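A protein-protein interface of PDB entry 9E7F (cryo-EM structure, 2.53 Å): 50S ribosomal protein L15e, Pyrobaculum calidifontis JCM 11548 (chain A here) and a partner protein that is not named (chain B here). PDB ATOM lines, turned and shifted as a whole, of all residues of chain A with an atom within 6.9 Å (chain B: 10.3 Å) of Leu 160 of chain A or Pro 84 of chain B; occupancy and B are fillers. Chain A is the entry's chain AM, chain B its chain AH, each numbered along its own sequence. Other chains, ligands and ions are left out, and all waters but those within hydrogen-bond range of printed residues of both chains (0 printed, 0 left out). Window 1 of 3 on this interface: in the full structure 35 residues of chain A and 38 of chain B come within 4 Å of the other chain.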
ATOM      1  N   VAL A 155      15.783  12.715  17.570  1.00  0.00           N
ATOM      2  CA  VAL A 155      14.591  13.379  18.072  1.00  0.00           C
ATOM      3  C   VAL A 155      13.950  14.085  16.884  1.00  0.00           C
ATOM      4  O   VAL A 155      14.653  14.716  16.091  1.00  0.00           O
ATOM      5  CB  VAL A 155      14.891  14.385  19.196  1.00  0.00           C
ATOM      6  CG1 VAL A 155      13.621  15.085  19.624  1.00  0.00           C
ATOM      7  CG2 VAL A 155      15.538  13.686  20.373  1.00  0.00           C
ATOM      8  N   PRO A 156      12.635  13.979  16.694  1.00  0.00           N
ATOM      9  CA  PRO A 156      11.988  14.702  15.595  1.00  0.00           C
ATOM     10  C   PRO A 156      12.099  16.204  15.794  1.00  0.00           C
ATOM     11  O   PRO A 156      12.098  16.702  16.920  1.00  0.00           O
ATOM     12  CB  PRO A 156      10.529  14.235  15.664  1.00  0.00           C
ATOM     13  CG  PRO A 156      10.534  13.019  16.514  1.00  0.00           C
ATOM     14  CD  PRO A 156      11.688  13.148  17.451  1.00  0.00           C
ATOM     15  N   ARG A 157      12.206  16.925  14.678  1.00  0.00           N
ATOM     16  CA  ARG A 157      12.301  18.378  14.753  1.00  0.00           C
ATOM     17  C   ARG A 157      11.012  18.997  15.272  1.00  0.00           C
ATOM     18  O   ARG A 157      11.041  20.091  15.846  1.00  0.00           O
ATOM     19  CB  ARG A 157      12.652  18.951  13.382  1.00  0.00           C
ATOM     20  CG  ARG A 157      12.920  20.444  13.387  1.00  0.00           C
ATOM     21  CD  ARG A 157      11.720  21.227  12.895  1.00  0.00           C
ATOM     22  NE  ARG A 157      12.116  22.432  12.181  1.00  0.00           N
ATOM     23  CZ  ARG A 157      12.638  23.505  12.759  1.00  0.00           C
ATOM     24  NH1 ARG A 157      12.831  23.560  14.065  1.00  0.00           N
ATOM     25  NH2 ARG A 157      12.980  24.546  12.008  1.00  0.00           N
ATOM     26  N   ARG A 158       9.876  18.321  15.081  1.00  0.00           N
ATOM     27  CA  ARG A 158       8.615  18.838  15.600  1.00  0.00           C
ATOM     28  C   ARG A 158       8.613  18.870  17.122  1.00  0.00           C
ATOM     29  O   ARG A 158       7.978  19.739  17.728  1.00  0.00           O
ATOM     30  CB  ARG A 158       7.439  18.005  15.080  1.00  0.00           C
ATOM     31  CG  ARG A 158       7.302  16.636  15.722  1.00  0.00           C
ATOM     32  CD  ARG A 158       6.669  15.641  14.779  1.00  0.00           C
ATOM     33  NE  ARG A 158       5.351  16.072  14.341  1.00  0.00           N
ATOM     34  CZ  ARG A 158       4.272  15.302  14.362  1.00  0.00           C
ATOM     35  NH1 ARG A 158       4.334  14.039  14.747  1.00  0.00           N
ATOM     36  NH2 ARG A 158       3.104  15.811  13.983  1.00  0.00           N
ATOM     37  N   ARG A 159       9.316  17.934  17.761  1.00  0.00           N
ATOM     38  CA  ARG A 159       9.320  17.900  19.218  1.00  0.00           C
ATOM     39  C   ARG A 159      10.099  19.075  19.789  1.00  0.00           C
ATOM     40  O   ARG A 159       9.640  19.745  20.720  1.00  0.00           O
ATOM     41  CB  ARG A 159       9.898  16.579  19.717  1.00  0.00           C
ATOM     42  CG  ARG A 159       9.377  16.175  21.080  1.00  0.00           C
ATOM     43  CD  ARG A 159       9.926  14.836  21.513  1.00  0.00           C
ATOM     44  NE  ARG A 159       9.261  13.738  20.829  1.00  0.00           N
ATOM     45  CZ  ARG A 159       9.510  12.458  21.058  1.00  0.00           C
ATOM     46  NH1 ARG A 159      10.397  12.079  21.961  1.00  0.00           N
ATOM     47  NH2 ARG A 159       8.852  11.535  20.368  1.00  0.00           N
ATOM     48  N   LEU A 160      11.283  19.342  19.245  1.00  0.00           N
ATOM     49  CA  LEU A 160      12.092  20.439  19.758  1.00  0.00           C
ATOM     50  C   LEU A 160      11.551  21.793  19.318  1.00  0.00           C
ATOM     51  O   LEU A 160      11.601  22.761  20.082  1.00  0.00           O
ATOM     52  CB  LEU A 160      13.540  20.277  19.309  1.00  0.00           C
ATOM     53  CG  LEU A 160      14.286  19.078  19.887  1.00  0.00           C
ATOM     54  CD1 LEU A 160      15.772  19.185  19.580  1.00  0.00           C
ATOM     55  CD2 LEU A 160      14.046  18.977  21.379  1.00  0.00           C
ATOM     56  N   ALA A 161      11.035  21.878  18.092  1.00  0.00           N
ATOM     57  CA  ALA A 161      10.571  23.159  17.573  1.00  0.00           C
ATOM     58  C   ALA A 161       9.279  23.604  18.245  1.00  0.00           C
ATOM     59  O   ALA A 161       9.092  24.797  18.505  1.00  0.00           O
ATOM     60  CB  ALA A 161      10.383  23.076  16.061  1.00  0.00           C
ATOM     61  N   ARG A 162       8.367  22.666  18.515  1.00  0.00           N
ATOM     62  CA  ARG A 162       7.086  23.036  19.110  1.00  0.00           C
ATOM     63  C   ARG A 162       7.252  23.538  20.537  1.00  0.00           C
ATOM     64  O   ARG A 162       6.657  24.552  20.919  1.00  0.00           O
ATOM     65  CB  ARG A 162       6.127  21.849  19.078  1.00  0.00           C
ATOM     66  CG  ARG A 162       4.914  22.042  19.958  1.00  0.00           C
ATOM     67  CD  ARG A 162       3.722  21.245  19.460  1.00  0.00           C
ATOM     68  NE  ARG A 162       3.935  19.813  19.614  1.00  0.00           N
ATOM     69  CZ  ARG A 162       3.078  18.985  20.192  1.00  0.00           C
ATOM     70  NH1 ARG A 162       1.934  19.418  20.696  1.00  0.00           N
ATOM     71  NH2 ARG A 162       3.377  17.693  20.270  1.00  0.00           N
ATOM     72  N   ARG A 163       8.053  22.840  21.344  1.00  0.00           N
ATOM     73  CA  ARG A 163       8.230  23.242  22.734  1.00  0.00           C
ATOM     74  C   ARG A 163       9.010  24.545  22.840  1.00  0.00           C
ATOM     75  O   ARG A 163       8.708  25.382  23.696  1.00  0.00           O
ATOM     76  CB  ARG A 163       8.932  22.136  23.515  1.00  0.00           C
ATOM     77  CG  ARG A 163       9.342  22.540  24.917  1.00  0.00           C
ATOM     78  CD  ARG A 163       8.303  22.113  25.923  1.00  0.00           C
ATOM     79  NE  ARG A 163       7.614  20.900  25.498  1.00  0.00           N
ATOM     80  CZ  ARG A 163       7.894  19.684  25.945  1.00  0.00           C
ATOM     81  NH1 ARG A 163       8.843  19.478  26.842  1.00  0.00           N
ATOM     82  NH2 ARG A 163       7.206  18.648  25.477  1.00  0.00           N
ATOM     83  N   LEU A 164      10.026  24.725  21.993  1.00  0.00           N
ATOM     84  CA  LEU A 164      10.777  25.977  21.991  1.00  0.00           C
ATOM     85  C   LEU A 164       9.895  27.145  21.573  1.00  0.00           C
ATOM     86  O   LEU A 164      10.021  28.250  22.109  1.00  0.00           O
ATOM     87  CB  LEU A 164      11.988  25.867  21.065  1.00  0.00           C
ATOM     88  CG  LEU A 164      13.299  25.354  21.664  1.00  0.00           C
ATOM     89  CD1 LEU A 164      14.409  25.409  20.635  1.00  0.00           C
ATOM     90  CD2 LEU A 164      13.691  26.143  22.898  1.00  0.00           C
ATOM     91  N   ARG A 165       9.006  26.920  20.602  1.00  0.00           N
ATOM     92  CA  ARG A 165       8.030  27.938  20.231  1.00  0.00           C
ATOM     93  C   ARG A 165       7.094  28.238  21.389  1.00  0.00           C
ATOM     94  O   ARG A 165       6.799  29.403  21.678  1.00  0.00           O
ATOM     95  CB  ARG A 165       7.225  27.482  19.017  1.00  0.00           C
ATOM     96  CG  ARG A 165       7.737  27.995  17.694  1.00  0.00           C
ATOM     97  CD  ARG A 165       6.687  27.846  16.616  1.00  0.00           C
ATOM     98  NE  ARG A 165       6.307  26.454  16.408  1.00  0.00           N
ATOM     99  CZ  ARG A 165       6.960  25.609  15.625  1.00  0.00           C
ATOM    100  NH1 ARG A 165       8.050  25.974  14.973  1.00  0.00           N
ATOM    101  NH2 ARG A 165       6.506  24.367  15.490  1.00  0.00           N
ATOM    102  N   ALA B  39      20.781  34.079  30.181  1.00  0.00           N
ATOM    103  CA  ALA B  39      21.133  33.431  28.920  1.00  0.00           C
ATOM    104  C   ALA B  39      19.967  32.630  28.357  1.00  0.00           C
ATOM    105  O   ALA B  39      19.719  32.657  27.148  1.00  0.00           O
ATOM    106  CB  ALA B  39      22.355  32.535  29.112  1.00  0.00           C
ATOM    107  N   GLU B  40      19.235  31.924  29.221  1.00  0.00           N
ATOM    108  CA  GLU B  40      18.111  31.112  28.762  1.00  0.00           C
ATOM    109  C   GLU B  40      16.998  31.978  28.184  1.00  0.00           C
ATOM    110  O   GLU B  40      16.460  31.681  27.113  1.00  0.00           O
ATOM    111  CB  GLU B  40      17.577  30.255  29.908  1.00  0.00           C
ATOM    112  CG  GLU B  40      17.971  28.792  29.835  1.00  0.00           C
ATOM    113  CD  GLU B  40      17.288  28.043  28.709  1.00  0.00           C
ATOM    114  OE1 GLU B  40      16.592  28.679  27.893  1.00  0.00           O
ATOM    115  OE2 GLU B  40      17.449  26.807  28.639  1.00  0.00           O
ATOM    116  N   ARG B  43      18.257  33.582  24.814  1.00  0.00           N
ATOM    117  CA  ARG B  43      18.243  32.618  23.719  1.00  0.00           C
ATOM    118  C   ARG B  43      16.821  32.229  23.341  1.00  0.00           C
ATOM    119  O   ARG B  43      16.543  31.945  22.171  1.00  0.00           O
ATOM    120  CB  ARG B  43      19.061  31.386  24.092  1.00  0.00           C
ATOM    121  CG  ARG B  43      20.550  31.626  24.074  1.00  0.00           C
ATOM    122  CD  ARG B  43      21.319  30.410  24.528  1.00  0.00           C
ATOM    123  NE  ARG B  43      22.747  30.684  24.587  1.00  0.00           N
ATOM    124  CZ  ARG B  43      23.557  30.233  25.532  1.00  0.00           C
ATOM    125  NH1 ARG B  43      23.115  29.455  26.506  1.00  0.00           N
ATOM    126  NH2 ARG B  43      24.842  30.567  25.498  1.00  0.00           N
ATOM    127  N   LEU B  44      15.907  32.199  24.314  1.00  0.00           N
ATOM    128  CA  LEU B  44      14.507  31.953  23.996  1.00  0.00           C
ATOM    129  C   LEU B  44      13.932  33.074  23.141  1.00  0.00           C
ATOM    130  O   LEU B  44      13.173  32.819  22.201  1.00  0.00           O
ATOM    131  CB  LEU B  44      13.699  31.786  25.282  1.00  0.00           C
ATOM    132  CG  LEU B  44      13.483  30.348  25.747  1.00  0.00           C
ATOM    133  CD1 LEU B  44      12.932  30.311  27.155  1.00  0.00           C
ATOM    134  CD2 LEU B  44      12.553  29.632  24.792  1.00  0.00           C
ATOM    135  N   GLU B  80      13.392  32.737  15.723  1.00  0.00           N
ATOM    136  CA  GLU B  80      13.327  31.477  16.440  1.00  0.00           C
ATOM    137  C   GLU B  80      14.446  31.414  17.478  1.00  0.00           C
ATOM    138  O   GLU B  80      15.474  32.078  17.331  1.00  0.00           O
ATOM    139  CB  GLU B  80      13.431  30.302  15.474  1.00  0.00           C
ATOM    140  CG  GLU B  80      14.526  30.441  14.435  1.00  0.00           C
ATOM    141  CD  GLU B  80      14.799  29.145  13.697  1.00  0.00           C
ATOM    142  OE1 GLU B  80      14.710  28.072  14.327  1.00  0.00           O
ATOM    143  OE2 GLU B  80      15.100  29.196  12.485  1.00  0.00           O
ATOM    144  N   PRO B  81      14.251  30.645  18.549  1.00  0.00           N
ATOM    145  CA  PRO B  81      15.213  30.658  19.658  1.00  0.00           C
ATOM    146  C   PRO B  81      16.575  30.114  19.255  1.00  0.00           C
ATOM    147  O   PRO B  81      16.693  29.228  18.409  1.00  0.00           O
ATOM    148  CB  PRO B  81      14.553  29.767  20.717  1.00  0.00           C
ATOM    149  CG  PRO B  81      13.144  29.605  20.293  1.00  0.00           C
ATOM    150  CD  PRO B  81      13.086  29.793  18.823  1.00  0.00           C
ATOM    151  N   THR B  82      17.613  30.662  19.886  1.00  0.00           N
ATOM    152  CA  THR B  82      18.997  30.300  19.584  1.00  0.00           C
ATOM    153  C   THR B  82      19.428  29.080  20.401  1.00  0.00           C
ATOM    154  O   THR B  82      20.392  29.104  21.164  1.00  0.00           O
ATOM    155  CB  THR B  82      19.915  31.486  19.842  1.00  0.00           C
ATOM    156  OG1 THR B  82      19.377  32.282  20.902  1.00  0.00           O
ATOM    157  CG2 THR B  82      20.043  32.337  18.599  1.00  0.00           C
ATOM    158  N   LEU B  83      18.694  27.995  20.213  1.00  0.00           N
ATOM    159  CA  LEU B  83      18.906  26.745  20.920  1.00  0.00           C
ATOM    160  C   LEU B  83      18.802  25.609  19.920  1.00  0.00           C
ATOM    161  O   LEU B  83      18.281  25.794  18.816  1.00  0.00           O
ATOM    162  CB  LEU B  83      17.885  26.559  22.050  1.00  0.00           C
ATOM    163  CG  LEU B  83      18.049  27.513  23.229  1.00  0.00           C
ATOM    164  CD1 LEU B  83      16.761  27.633  23.998  1.00  0.00           C
ATOM    165  CD2 LEU B  83      19.156  27.037  24.136  1.00  0.00           C
ATOM    166  N   PRO B  84      19.323  24.433  20.260  1.00  0.00           N
ATOM    167  CA  PRO B  84      19.263  23.301  19.325  1.00  0.00           C
ATOM    168  C   PRO B  84      17.828  22.867  19.050  1.00  0.00           C
ATOM    169  O   PRO B  84      17.050  22.602  19.968  1.00  0.00           O
ATOM    170  CB  PRO B  84      20.062  22.199  20.032  1.00  0.00           C
ATOM    171  CG  PRO B  84      20.666  22.797  21.228  1.00  0.00           C
ATOM    172  CD  PRO B  84      20.204  24.192  21.412  1.00  0.00           C
ATOM    173  N   LYS B  85      17.489  22.793  17.763  1.00  0.00           N
ATOM    174  CA  LYS B  85      16.163  22.401  17.321  1.00  0.00           C
ATOM    175  C   LYS B  85      16.121  21.017  16.691  1.00  0.00           C
ATOM    176  O   LYS B  85      15.059  20.608  16.216  1.00  0.00           O
ATOM    177  CB  LYS B  85      15.616  23.420  16.312  1.00  0.00           C
ATOM    178  CG  LYS B  85      15.942  24.859  16.639  1.00  0.00           C
ATOM    179  CD  LYS B  85      16.309  25.626  15.381  1.00  0.00           C
ATOM    180  CE  LYS B  85      17.115  26.871  15.703  1.00  0.00           C
ATOM    181  NZ  LYS B  85      18.504  26.557  16.121  1.00  0.00           N
ATOM    182  N   VAL B  86      17.237  20.300  16.650  1.00  0.00           N
ATOM    183  CA  VAL B  86      17.277  18.951  16.102  1.00  0.00           C
ATOM    184  C   VAL B  86      18.345  18.158  16.838  1.00  0.00           C
ATOM    185  O   VAL B  86      19.366  18.711  17.259  1.00  0.00           O
ATOM    186  CB  VAL B  86      17.542  18.961  14.583  1.00  0.00           C
ATOM    187  CG1 VAL B  86      19.026  19.071  14.296  1.00  0.00           C
ATOM    188  CG2 VAL B  86      16.967  17.712  13.947  1.00  0.00           C
ATOM    189  N   VAL B  87      18.101  16.862  17.009  1.00  0.00           N
ATOM    190  CA  VAL B  87      19.034  15.958  17.669  1.00  0.00           C
ATOM    191  C   VAL B  87      19.258  14.786  16.724  1.00  0.00           C
ATOM    192  O   VAL B  87      18.431  13.874  16.651  1.00  0.00           O
ATOM    193  CB  VAL B  87      18.522  15.475  19.028  1.00  0.00           C
ATOM    194  CG1 VAL B  87      19.636  14.791  19.796  1.00  0.00           C
ATOM    195  CG2 VAL B  87      17.947  16.633  19.821  1.00  0.00           C
ATOM    196  N   LYS B  88      20.370  14.803  16.001  1.00  0.00           N
ATOM    197  CA  LYS B  88      20.725  13.723  15.086  1.00  0.00           C
ATOM    198  C   LYS B  88      22.079  13.167  15.508  1.00  0.00           C
ATOM    199  O   LYS B  88      23.117  13.782  15.252  1.00  0.00           O
ATOM    200  CB  LYS B  88      20.750  14.209  13.644  1.00  0.00           C
ATOM    201  CG  LYS B  88      20.649  13.093  12.626  1.00  0.00           C
ATOM    202  CD  LYS B  88      20.740  13.622  11.204  1.00  0.00           C
ATOM    203  CE  LYS B  88      20.314  15.077  11.124  1.00  0.00           C
ATOM    204  NZ  LYS B  88      20.298  15.577   9.721  1.00  0.00           N
ATOM    205  N   VAL B  89      22.070  12.006  16.154  1.00  0.00           N
ATOM    206  CA  VAL B  89      23.288  11.301  16.528  1.00  0.00           C
ATOM    207  C   VAL B  89      23.281   9.954  15.823  1.00  0.00           C
ATOM    208  O   VAL B  89      22.391   9.129  16.059  1.00  0.00           O
ATOM    209  CB  VAL B  89      23.409  11.129  18.048  1.00  0.00           C
ATOM    210  CG1 VAL B  89      24.718  10.451  18.393  1.00  0.00           C
ATOM    211  CG2 VAL B  89      23.313  12.473  18.732  1.00  0.00           C
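CG of Arg 157 of chain A touches O of Lys 85 of chain B, at 3.6 Å. Leu 160 of chain A touches Pro 84 of chain B. Leu 160 of chain A touches Lys 85 of chain B. Leu 160 of chain A touches Val 86 of chain B (CD1 to N, 3.5 Å). CG2 of Val 87 of chain B touches CD1 of Leu 160 of chain A, 3.4 Å away. Leu 164 of chain A touches Leu 44 of chain B (O to CD2, 3.9 Å). Leu 164 of chain A touches Pro 81 of chain B (O to CG, 3.9 Å). Leu 83 of chain B touches Leu 164 of chain A (CD1 to CD2, 3.6 Å). O of Pro 84 of chain B touches CD1 of Leu 164 of chain A (3.9 Å).
The backbone NH (N) of Val 155 of chain A sits at hydrogen-bond distance from the backbone carbonyl oxygen (O) of Val 87 of chain B, at 3.0 Å.
O of Leu 83 of chain B lies within hydrogen-bond range of NZ of Lys 85 of chain B, 2.8 Å away.
Leu 160 of chain A touches just these residues of chain B: Pro 84 (3.7 Å), Lys 85 (3.4 Å), Val 86 (3.5 Å) and Val 87 (3.4 Å). Printed residues of chain A within 4 Å of Pro 84 of chain B: Leu 160 and Leu 164. No residue of chain B comes within 4 Å of Ala 161 of chain A. Leu 164 of chain A touches just these residues of chain B: Leu 44 (3.9 Å), Pro 81 (3.9 Å), Leu 83 (3.6 Å) and Pro 84 (3.9 Å). Of the printed residues of chain A, Pro 81 of chain B touches Leu 164. Printed residues of chain A within 4 Å of Leu 44 of chain B: Leu 164. Printed residues of chain B within 4 Å of Val 155 of chain A: Val 87. Of the printed residues of chain A, Leu 83 of chain B touches Leu 164 (3.6 Å). Arg 159 of chain A touches none of the printed residues of chain B. Ala 39 of chain B touches none of the printed residues of chain A. The nearest residue of chain B that does not touch Leu 160 of chain A is Pro 81 of chain B (7.0 Å). The nearest residue of chain A that does not touch Pro 84 of chain B is Ala 161 of chain A (6.3 Å). The nearest printed residue of chain A that does not touch Pro 81 of chain B is Arg 165 of chain A (4.9 Å).
Hydrophobic or aromatic side chains of chain A that line the printed part of chain B: Val 155, Leu 160 and Leu 164. Among the printed residues, no Asp or Glu carboxylate lies within 4 Å of a Lys or Arg side-chain nitrogen of the other chain.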
